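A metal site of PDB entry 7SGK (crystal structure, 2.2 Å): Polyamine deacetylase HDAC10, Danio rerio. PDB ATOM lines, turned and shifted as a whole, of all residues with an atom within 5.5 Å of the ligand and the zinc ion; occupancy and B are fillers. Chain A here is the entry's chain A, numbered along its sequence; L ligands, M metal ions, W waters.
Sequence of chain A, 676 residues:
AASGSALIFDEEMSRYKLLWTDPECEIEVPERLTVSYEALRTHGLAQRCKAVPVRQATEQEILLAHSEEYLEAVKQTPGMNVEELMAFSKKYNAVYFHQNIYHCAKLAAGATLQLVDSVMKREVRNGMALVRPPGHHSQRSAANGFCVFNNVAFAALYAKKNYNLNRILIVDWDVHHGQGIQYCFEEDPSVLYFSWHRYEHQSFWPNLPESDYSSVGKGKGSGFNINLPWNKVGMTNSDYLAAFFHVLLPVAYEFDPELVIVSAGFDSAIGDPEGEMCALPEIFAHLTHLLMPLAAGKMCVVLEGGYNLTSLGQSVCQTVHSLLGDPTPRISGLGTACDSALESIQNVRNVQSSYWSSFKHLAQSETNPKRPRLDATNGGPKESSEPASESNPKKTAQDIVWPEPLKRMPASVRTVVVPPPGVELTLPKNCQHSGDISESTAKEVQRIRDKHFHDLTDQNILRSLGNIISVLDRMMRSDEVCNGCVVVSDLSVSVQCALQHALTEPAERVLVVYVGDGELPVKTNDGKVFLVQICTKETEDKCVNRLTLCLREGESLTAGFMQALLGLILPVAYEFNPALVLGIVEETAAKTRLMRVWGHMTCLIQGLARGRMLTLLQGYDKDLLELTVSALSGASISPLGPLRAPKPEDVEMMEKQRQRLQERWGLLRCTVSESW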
ATOM      1  N   GLU A  24     -33.981 -13.642  33.393  1.00  0.00           N
ATOM      2  CA  GLU A  24     -32.928 -13.069  32.574  1.00  0.00           C
ATOM      3  C   GLU A  24     -31.741 -12.593  33.412  1.00  0.00           C
ATOM      4  O   GLU A  24     -30.582 -12.679  32.965  1.00  0.00           O
ATOM      5  CB  GLU A  24     -33.501 -11.928  31.738  1.00  0.00           C
ATOM      6  CG  GLU A  24     -32.720 -11.633  30.471  1.00  0.00           C
ATOM      7  CD  GLU A  24     -33.388 -10.608  29.569  1.00  0.00           C
ATOM      8  OE1 GLU A  24     -34.425 -10.023  29.963  1.00  0.00           O
ATOM      9  OE2 GLU A  24     -32.844 -10.373  28.458  1.00  0.00           O
ATOM     10  N   ILE A  27     -28.947 -14.793  37.230  1.00  0.00           N
ATOM     11  CA  ILE A  27     -27.625 -15.393  37.295  1.00  0.00           C
ATOM     12  C   ILE A  27     -26.588 -14.419  37.808  1.00  0.00           C
ATOM     13  O   ILE A  27     -25.499 -14.842  38.207  1.00  0.00           O
ATOM     14  CB  ILE A  27     -27.150 -15.918  35.931  1.00  0.00           C
ATOM     15  CG1 ILE A  27     -27.408 -14.870  34.848  1.00  0.00           C
ATOM     16  CG2 ILE A  27     -27.787 -17.249  35.596  1.00  0.00           C
ATOM     17  CD1 ILE A  27     -26.447 -14.957  33.694  1.00  0.00           C
ATOM     18  N   ALA A  94     -32.237  -6.231  29.978  1.00  0.00           N
ATOM     19  CA  ALA A  94     -31.438  -7.204  30.723  1.00  0.00           C
ATOM     20  C   ALA A  94     -30.582  -6.533  31.802  1.00  0.00           C
ATOM     21  O   ALA A  94     -29.365  -6.691  31.860  1.00  0.00           O
ATOM     22  CB  ALA A  94     -30.569  -8.022  29.759  1.00  0.00           C
ATOM     23  N   HIS A 136     -19.207  -3.738  30.310  1.00  0.00           N
ATOM     24  CA  HIS A 136     -18.890  -3.623  28.869  1.00  0.00           C
ATOM     25  C   HIS A 136     -20.123  -3.447  27.978  1.00  0.00           C
ATOM     26  O   HIS A 136     -19.956  -2.988  26.842  1.00  0.00           O
ATOM     27  CB  HIS A 136     -18.038  -4.793  28.354  1.00  0.00           C
ATOM     28  CG  HIS A 136     -18.709  -6.144  28.340  1.00  0.00           C
ATOM     29  ND1 HIS A 136     -18.290  -7.164  27.513  1.00  0.00           N
ATOM     30  CD2 HIS A 136     -19.720  -6.645  29.084  1.00  0.00           C
ATOM     31  CE1 HIS A 136     -19.019  -8.241  27.743  1.00  0.00           C
ATOM     32  NE2 HIS A 136     -19.880  -7.955  28.717  1.00  0.00           N
ATOM     33  N   HIS A 137     -21.328  -3.738  28.459  1.00  0.00           N
ATOM     34  CA  HIS A 137     -22.545  -3.500  27.692  1.00  0.00           C
ATOM     35  C   HIS A 137     -23.083  -2.093  27.867  1.00  0.00           C
ATOM     36  O   HIS A 137     -23.919  -1.665  27.061  1.00  0.00           O
ATOM     37  CB  HIS A 137     -23.640  -4.487  28.108  1.00  0.00           C
ATOM     38  CG  HIS A 137     -23.299  -5.907  27.799  1.00  0.00           C
ATOM     39  ND1 HIS A 137     -22.843  -6.307  26.560  1.00  0.00           N
ATOM     40  CD2 HIS A 137     -23.325  -7.019  28.569  1.00  0.00           C
ATOM     41  CE1 HIS A 137     -22.616  -7.603  26.581  1.00  0.00           C
ATOM     42  NE2 HIS A 137     -22.894  -8.062  27.786  1.00  0.00           N
ATOM     43  N   GLY A 145     -27.479  -5.166  29.926  1.00  0.00           N
ATOM     44  CA  GLY A 145     -26.773  -6.410  30.180  1.00  0.00           C
ATOM     45  C   GLY A 145     -26.032  -6.493  31.506  1.00  0.00           C
ATOM     46  O   GLY A 145     -24.844  -6.846  31.545  1.00  0.00           O
ATOM     47  N   PHE A 146     -26.731  -6.155  32.604  1.00  0.00           N
ATOM     48  CA  PHE A 146     -26.214  -6.111  33.980  1.00  0.00           C
ATOM     49  C   PHE A 146     -25.293  -4.922  34.216  1.00  0.00           C
ATOM     50  O   PHE A 146     -24.866  -4.692  35.352  1.00  0.00           O
ATOM     51  CB  PHE A 146     -25.442  -7.391  34.362  1.00  0.00           C
ATOM     52  CG  PHE A 146     -26.162  -8.670  34.008  1.00  0.00           C
ATOM     53  CD1 PHE A 146     -27.544  -8.729  33.994  1.00  0.00           C
ATOM     54  CD2 PHE A 146     -25.439  -9.819  33.720  1.00  0.00           C
ATOM     55  CE1 PHE A 146     -28.206  -9.896  33.679  1.00  0.00           C
ATOM     56  CE2 PHE A 146     -26.100 -10.995  33.416  1.00  0.00           C
ATOM     57  CZ  PHE A 146     -27.481 -11.023  33.391  1.00  0.00           C
ATOM     58  N   ASP A 174     -14.915 -11.942  27.349  1.00  0.00           N
ATOM     59  CA  ASP A 174     -16.266 -12.296  27.760  1.00  0.00           C
ATOM     60  C   ASP A 174     -16.985 -12.968  26.598  1.00  0.00           C
ATOM     61  O   ASP A 174     -16.635 -12.768  25.428  1.00  0.00           O
ATOM     62  CB  ASP A 174     -17.003 -11.026  28.215  1.00  0.00           C
ATOM     63  CG  ASP A 174     -18.303 -11.291  28.962  1.00  0.00           C
ATOM     64  OD1 ASP A 174     -18.314 -11.166  30.203  1.00  0.00           O
ATOM     65  OD2 ASP A 174     -19.329 -11.610  28.326  1.00  0.00           O
ATOM     66  N   VAL A 175     -17.987 -13.805  26.906  1.00  0.00           N
ATOM     67  CA  VAL A 175     -18.686 -14.523  25.842  1.00  0.00           C
ATOM     68  C   VAL A 175     -19.704 -13.648  25.136  1.00  0.00           C
ATOM     69  O   VAL A 175     -20.172 -13.995  24.047  1.00  0.00           O
ATOM     70  CB  VAL A 175     -19.353 -15.800  26.379  1.00  0.00           C
ATOM     71  CG1 VAL A 175     -20.690 -15.486  27.056  1.00  0.00           C
ATOM     72  CG2 VAL A 175     -19.517 -16.845  25.235  1.00  0.00           C
ATOM     73  N   HIS A 176     -20.066 -12.515  25.726  1.00  0.00           N
ATOM     74  CA  HIS A 176     -20.978 -11.555  25.141  1.00  0.00           C
ATOM     75  C   HIS A 176     -20.210 -10.424  24.498  1.00  0.00           C
ATOM     76  O   HIS A 176     -19.083 -10.105  24.900  1.00  0.00           O
ATOM     77  CB  HIS A 176     -21.945 -11.009  26.196  1.00  0.00           C
ATOM     78  CG  HIS A 176     -22.819 -12.053  26.814  1.00  0.00           C
ATOM     79  ND1 HIS A 176     -22.459 -12.746  27.958  1.00  0.00           N
ATOM     80  CD2 HIS A 176     -24.014 -12.567  26.426  1.00  0.00           C
ATOM     81  CE1 HIS A 176     -23.415 -13.610  28.256  1.00  0.00           C
ATOM     82  NE2 HIS A 176     -24.360 -13.523  27.347  1.00  0.00           N
ATOM     83  N   ARG A 198     -20.232 -15.198  21.539  1.00  0.00           N
ATOM     84  CA  ARG A 198     -21.327 -15.999  21.038  1.00  0.00           C
ATOM     85  C   ARG A 198     -22.275 -15.096  20.254  1.00  0.00           C
ATOM     86  O   ARG A 198     -22.755 -14.077  20.782  1.00  0.00           O
ATOM     87  CB  ARG A 198     -22.049 -16.669  22.197  1.00  0.00           C
ATOM     88  CG  ARG A 198     -23.228 -17.532  21.803  1.00  0.00           C
ATOM     89  CD  ARG A 198     -23.815 -18.256  22.992  1.00  0.00           C
ATOM     90  NE  ARG A 198     -24.976 -19.026  22.599  1.00  0.00           N
ATOM     91  CZ  ARG A 198     -25.731 -19.747  23.416  1.00  0.00           C
ATOM     92  NH1 ARG A 198     -25.467 -19.794  24.710  1.00  0.00           N
ATOM     93  NH2 ARG A 198     -26.778 -20.422  22.921  1.00  0.00           N
ATOM     94  N   PHE A 204     -28.118 -14.782  19.057  1.00  0.00           N
ATOM     95  CA  PHE A 204     -27.795 -14.708  20.472  1.00  0.00           C
ATOM     96  C   PHE A 204     -27.654 -13.264  20.944  1.00  0.00           C
ATOM     97  O   PHE A 204     -27.039 -12.428  20.278  1.00  0.00           O
ATOM     98  CB  PHE A 204     -26.514 -15.476  20.801  1.00  0.00           C
ATOM     99  CG  PHE A 204     -26.307 -15.663  22.273  1.00  0.00           C
ATOM    100  CD1 PHE A 204     -27.103 -16.561  22.984  1.00  0.00           C
ATOM    101  CD2 PHE A 204     -25.346 -14.923  22.962  1.00  0.00           C
ATOM    102  CE1 PHE A 204     -26.932 -16.719  24.356  1.00  0.00           C
ATOM    103  CE2 PHE A 204     -25.168 -15.099  24.336  1.00  0.00           C
ATOM    104  CZ  PHE A 204     -25.965 -15.988  25.036  1.00  0.00           C
ATOM    105  N   TRP A 205     -28.237 -13.005  22.110  1.00  0.00           N
ATOM    106  CA  TRP A 205     -28.214 -11.704  22.745  1.00  0.00           C
ATOM    107  C   TRP A 205     -26.800 -11.123  22.728  1.00  0.00           C
ATOM    108  O   TRP A 205     -25.841 -11.840  23.037  1.00  0.00           O
ATOM    109  CB  TRP A 205     -28.743 -11.833  24.182  1.00  0.00           C
ATOM    110  CG  TRP A 205     -28.978 -10.519  24.823  1.00  0.00           C
ATOM    111  CD1 TRP A 205     -30.160  -9.843  24.887  1.00  0.00           C
ATOM    112  CD2 TRP A 205     -28.013  -9.717  25.480  1.00  0.00           C
ATOM    113  NE1 TRP A 205     -29.977  -8.653  25.539  1.00  0.00           N
ATOM    114  CE2 TRP A 205     -28.660  -8.547  25.896  1.00  0.00           C
ATOM    115  CE3 TRP A 205     -26.642  -9.861  25.725  1.00  0.00           C
ATOM    116  CZ2 TRP A 205     -27.985  -7.516  26.576  1.00  0.00           C
ATOM    117  CZ3 TRP A 205     -25.979  -8.847  26.392  1.00  0.00           C
ATOM    118  CH2 TRP A 205     -26.655  -7.688  26.813  1.00  0.00           C
ATOM    119  N   ASP A 267     -17.704 -16.034  31.502  1.00  0.00           N
ATOM    120  CA  ASP A 267     -18.782 -16.815  30.933  1.00  0.00           C
ATOM    121  C   ASP A 267     -18.375 -17.476  29.630  1.00  0.00           C
ATOM    122  O   ASP A 267     -19.190 -18.097  28.958  1.00  0.00           O
ATOM    123  CB  ASP A 267     -20.052 -15.975  30.737  1.00  0.00           C
ATOM    124  CG  ASP A 267     -19.766 -14.595  30.167  1.00  0.00           C
ATOM    125  OD1 ASP A 267     -18.643 -14.345  29.680  1.00  0.00           O
ATOM    126  OD2 ASP A 267     -20.694 -13.774  30.208  1.00  0.00           O
ATOM    127  N   PRO A 273     -23.676 -21.238  32.043  1.00  0.00           N
ATOM    128  CA  PRO A 273     -24.991 -21.406  31.413  1.00  0.00           C
ATOM    129  C   PRO A 273     -25.270 -20.388  30.326  1.00  0.00           C
ATOM    130  O   PRO A 273     -26.160 -20.624  29.502  1.00  0.00           O
ATOM    131  CB  PRO A 273     -25.971 -21.249  32.580  1.00  0.00           C
ATOM    132  CG  PRO A 273     -25.242 -20.265  33.519  1.00  0.00           C
ATOM    133  CD  PRO A 273     -23.762 -20.605  33.384  1.00  0.00           C
ATOM    134  N   GLU A 274     -24.573 -19.255  30.312  1.00  0.00           N
ATOM    135  CA  GLU A 274     -24.768 -18.218  29.315  1.00  0.00           C
ATOM    136  C   GLU A 274     -23.963 -18.470  28.062  1.00  0.00           C
ATOM    137  O   GLU A 274     -24.456 -18.239  26.957  1.00  0.00           O
ATOM    138  CB  GLU A 274     -24.365 -16.841  29.864  1.00  0.00           C
ATOM    139  CG  GLU A 274     -25.478 -16.158  30.617  1.00  0.00           C
ATOM    140  CD  GLU A 274     -26.566 -15.651  29.715  1.00  0.00           C
ATOM    141  OE1 GLU A 274     -26.241 -15.051  28.658  1.00  0.00           O
ATOM    142  OE2 GLU A 274     -27.761 -15.860  30.041  1.00  0.00           O
ATOM    143  N   GLU A 276     -22.053 -21.459  27.158  1.00  0.00           N
ATOM    144  CA  GLU A 276     -22.152 -22.826  26.653  1.00  0.00           C
ATOM    145  C   GLU A 276     -20.923 -23.216  25.842  1.00  0.00           C
ATOM    146  O   GLU A 276     -20.984 -24.066  24.958  1.00  0.00           O
ATOM    147  CB  GLU A 276     -23.440 -23.026  25.834  1.00  0.00           C
ATOM    148  CG  GLU A 276     -24.723 -23.017  26.677  1.00  0.00           C
ATOM    149  CD  GLU A 276     -25.984 -23.063  25.808  1.00  0.00           C
ATOM    150  OE1 GLU A 276     -25.884 -23.582  24.671  1.00  0.00           O
ATOM    151  OE2 GLU A 276     -27.063 -22.586  26.238  1.00  0.00           O
ATOM    152  N   GLU A 304     -15.764  -8.932  34.143  1.00  0.00           N
ATOM    153  CA  GLU A 304     -17.054  -8.670  33.533  1.00  0.00           C
ATOM    154  C   GLU A 304     -18.014  -9.752  34.002  1.00  0.00           C
ATOM    155  O   GLU A 304     -18.483  -9.698  35.158  1.00  0.00           O
ATOM    156  CB  GLU A 304     -16.933  -8.594  32.002  1.00  0.00           C
ATOM    157  CG  GLU A 304     -16.003  -7.505  31.507  1.00  0.00           C
ATOM    158  CD  GLU A 304     -16.674  -6.146  31.399  1.00  0.00           C
ATOM    159  OE1 GLU A 304     -17.883  -6.044  31.682  1.00  0.00           O
ATOM    160  OE2 GLU A 304     -15.995  -5.170  31.008  1.00  0.00           O
ATOM    161  N   GLY A 305     -18.345 -10.748  33.168  1.00  0.00           N
ATOM    162  CA  GLY A 305     -19.264 -11.795  33.531  1.00  0.00           C
ATOM    163  C   GLY A 305     -18.574 -13.080  33.947  1.00  0.00           C
ATOM    164  O   GLY A 305     -17.364 -13.127  34.154  1.00  0.00           O
ATOM    165  N   GLY A 306     -19.378 -14.146  34.038  1.00  0.00           N
ATOM    166  CA  GLY A 306     -18.954 -15.471  34.501  1.00  0.00           C
ATOM    167  C   GLY A 306     -19.855 -15.920  35.635  1.00  0.00           C
ATOM    168  O   GLY A 306     -19.816 -15.344  36.728  1.00  0.00           O
ATOM    169  N   TYR A 307     -20.687 -16.939  35.392  1.00  0.00           N
ATOM    170  CA  TYR A 307     -21.818 -17.192  36.255  1.00  0.00           C
ATOM    171  C   TYR A 307     -21.882 -18.595  36.853  1.00  0.00           C
ATOM    172  O   TYR A 307     -22.685 -18.819  37.764  1.00  0.00           O
ATOM    173  CB  TYR A 307     -23.124 -16.899  35.498  1.00  0.00           C
ATOM    174  CG  TYR A 307     -23.050 -15.525  34.904  1.00  0.00           C
ATOM    175  CD1 TYR A 307     -23.271 -14.404  35.688  1.00  0.00           C
ATOM    176  CD2 TYR A 307     -22.684 -15.346  33.584  1.00  0.00           C
ATOM    177  CE1 TYR A 307     -23.168 -13.140  35.165  1.00  0.00           C
ATOM    178  CE2 TYR A 307     -22.589 -14.077  33.039  1.00  0.00           C
ATOM    179  CZ  TYR A 307     -22.836 -12.975  33.828  1.00  0.00           C
ATOM    180  OH  TYR A 307     -22.731 -11.711  33.295  1.00  0.00           O
HETATM  181  C1  LIG L   1     -29.121 -11.946  28.616  1.00  0.00           C
HETATM  182  N1  LIG L   1     -28.504 -14.250  27.824  1.00  0.00           N
HETATM  183  C2  LIG L   1     -29.327 -15.177  27.027  1.00  0.00           C
HETATM  184  C3  LIG L   1     -29.373 -16.693  27.315  1.00  0.00           C
HETATM  185  C4  LIG L   1     -28.234 -18.848  27.395  1.00  0.00           C
HETATM  186  C5  LIG L   1     -30.551 -17.317  27.711  1.00  0.00           C
HETATM  187  C6  LIG L   1     -27.955 -12.794  30.508  1.00  0.00           C
HETATM  188  C7  LIG L   1     -26.997 -10.945  29.256  1.00  0.00           C
HETATM  189  C8  LIG L   1     -25.715 -11.484  29.904  1.00  0.00           C
HETATM  190  C9  LIG L   1     -24.757 -10.369  30.314  1.00  0.00           C
HETATM  191  C10 LIG L   1     -23.274 -10.788  30.315  1.00  0.00           C
HETATM  192  C11 LIG L   1     -28.422 -12.814  27.567  1.00  0.00           C
HETATM  193  C12 LIG L   1     -28.220 -17.476  27.167  1.00  0.00           C
HETATM  194  C13 LIG L   1     -29.408 -19.458  27.802  1.00  0.00           C
HETATM  195  C14 LIG L   1     -30.567 -18.688  27.949  1.00  0.00           C
HETATM  196  N2  LIG L   1     -28.222 -11.621  29.716  1.00  0.00           N
HETATM  197  N3  LIG L   1     -22.356  -9.903  29.671  1.00  0.00           N
HETATM  198  O1  LIG L   1     -22.847 -11.789  30.788  1.00  0.00           O
HETATM  199  O2  LIG L   1     -21.004 -10.215  29.631  1.00  0.00           O
HETATM  200  O3  LIG L   1     -29.961 -14.740  26.121  1.00  0.00           O
HETATM  201 ZN    ZN M   1     -20.839 -12.002  29.390  1.00  0.00          ZN
HETATM  202  O   HOH W   1     -30.274 -14.741  23.130  1.00  0.00           O
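Water W1 lies within hydrogen-bond range of N of Trp 205 (2.9 Å) and O3 of the ligand (3.0 Å).
The zinc ion is bound by an oxygen (O2) of the ligand (1.8 Å), the side-chain carboxylate of Asp 174 (1.9 Å), the side-chain carboxylate of Asp 267 (2.0 Å), a ring nitrogen (ND1) of His 176 (2.3 Å) and an oxygen (O1) of the ligand (2.5 Å).
Slightly farther from the zinc ion lies OD1 of Asp 174 (2.8 Å).
Along chain A the residues within 4 Å of the zinc ion span positions 174 to 267.
The side-chain carboxylate of Asp 174 is in hydrogen-bond range of the backbone NH of Gly 305 (3.0 Å).
A ring nitrogen (NE2) of His 176 lies within hydrogen-bond range of the side-chain carboxylate (OE1) of Glu 274.
The guanidinium group (NH1) of Arg 198 lies within hydrogen-bond range of the backbone carbonyl oxygen (O) of Glu 274, at 2.9 Å.
A ring nitrogen (NE2) of His 136 sits at hydrogen-bond distance from a ring nitrogen (NE2) of His 137 (3.2 Å).
O of Ala 94 sits at hydrogen-bond distance from N of Phe 146 (2.8 Å).
O of Ala 94 sits at hydrogen-bond distance from N of Gly 145.
The guanidinium group (NH1) of Arg 198 is in salt-bridge range of the side-chain carboxylate (OE2) of Glu 276, 3.6 Å away.
The backbone carbonyl oxygen of Val 175 lies within hydrogen-bond range of the backbone NH of Arg 198 (2.8 Å).
Residues that only touch the ligand: Phe 204 (3.2 Å), Phe 146 (3.4 Å), Pro 273 (3.4 Å), Trp 205 (3.5 Å), Glu 24 (3.6 Å), Gly 145 (3.7 Å) and Arg 198 (3.97 Å).
Hydrophobic or aromatic side chains within 4 Å of the ligand: His 136, His 137, Phe 146, His 176, Phe 204, Trp 205 and Tyr 307.
Within 4 Å of the ligand: Glu 24, His 136, His 137, Gly 145, Phe 146, Asp 174, His 176, Arg 198, Phe 204, Trp 205, Asp 267, Pro 273, Glu 274 and Tyr 307.
Along chain A the residues within 4 Å of the ligand span positions 24 to 307.
The nearest printed residue that does not touch the ligand is Glu 276 (4.1 Å).
The side-chain hydroxyl (OH) of Tyr 307 lies close to an oxygen (O1) of the ligand (2.5 Å).
The side-chain carboxylate (OE1) of Glu 274 is in hydrogen-bond range of a nitrogen (N1) of the ligand, 2.5 Å away.
A ring nitrogen (NE2) of His 136 is in hydrogen-bond range of a nitrogen (N3) of the ligand (3.3 Å).
N3 of the ligand lies within hydrogen-bond range of NE2 of His 137, 2.7 Å away.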
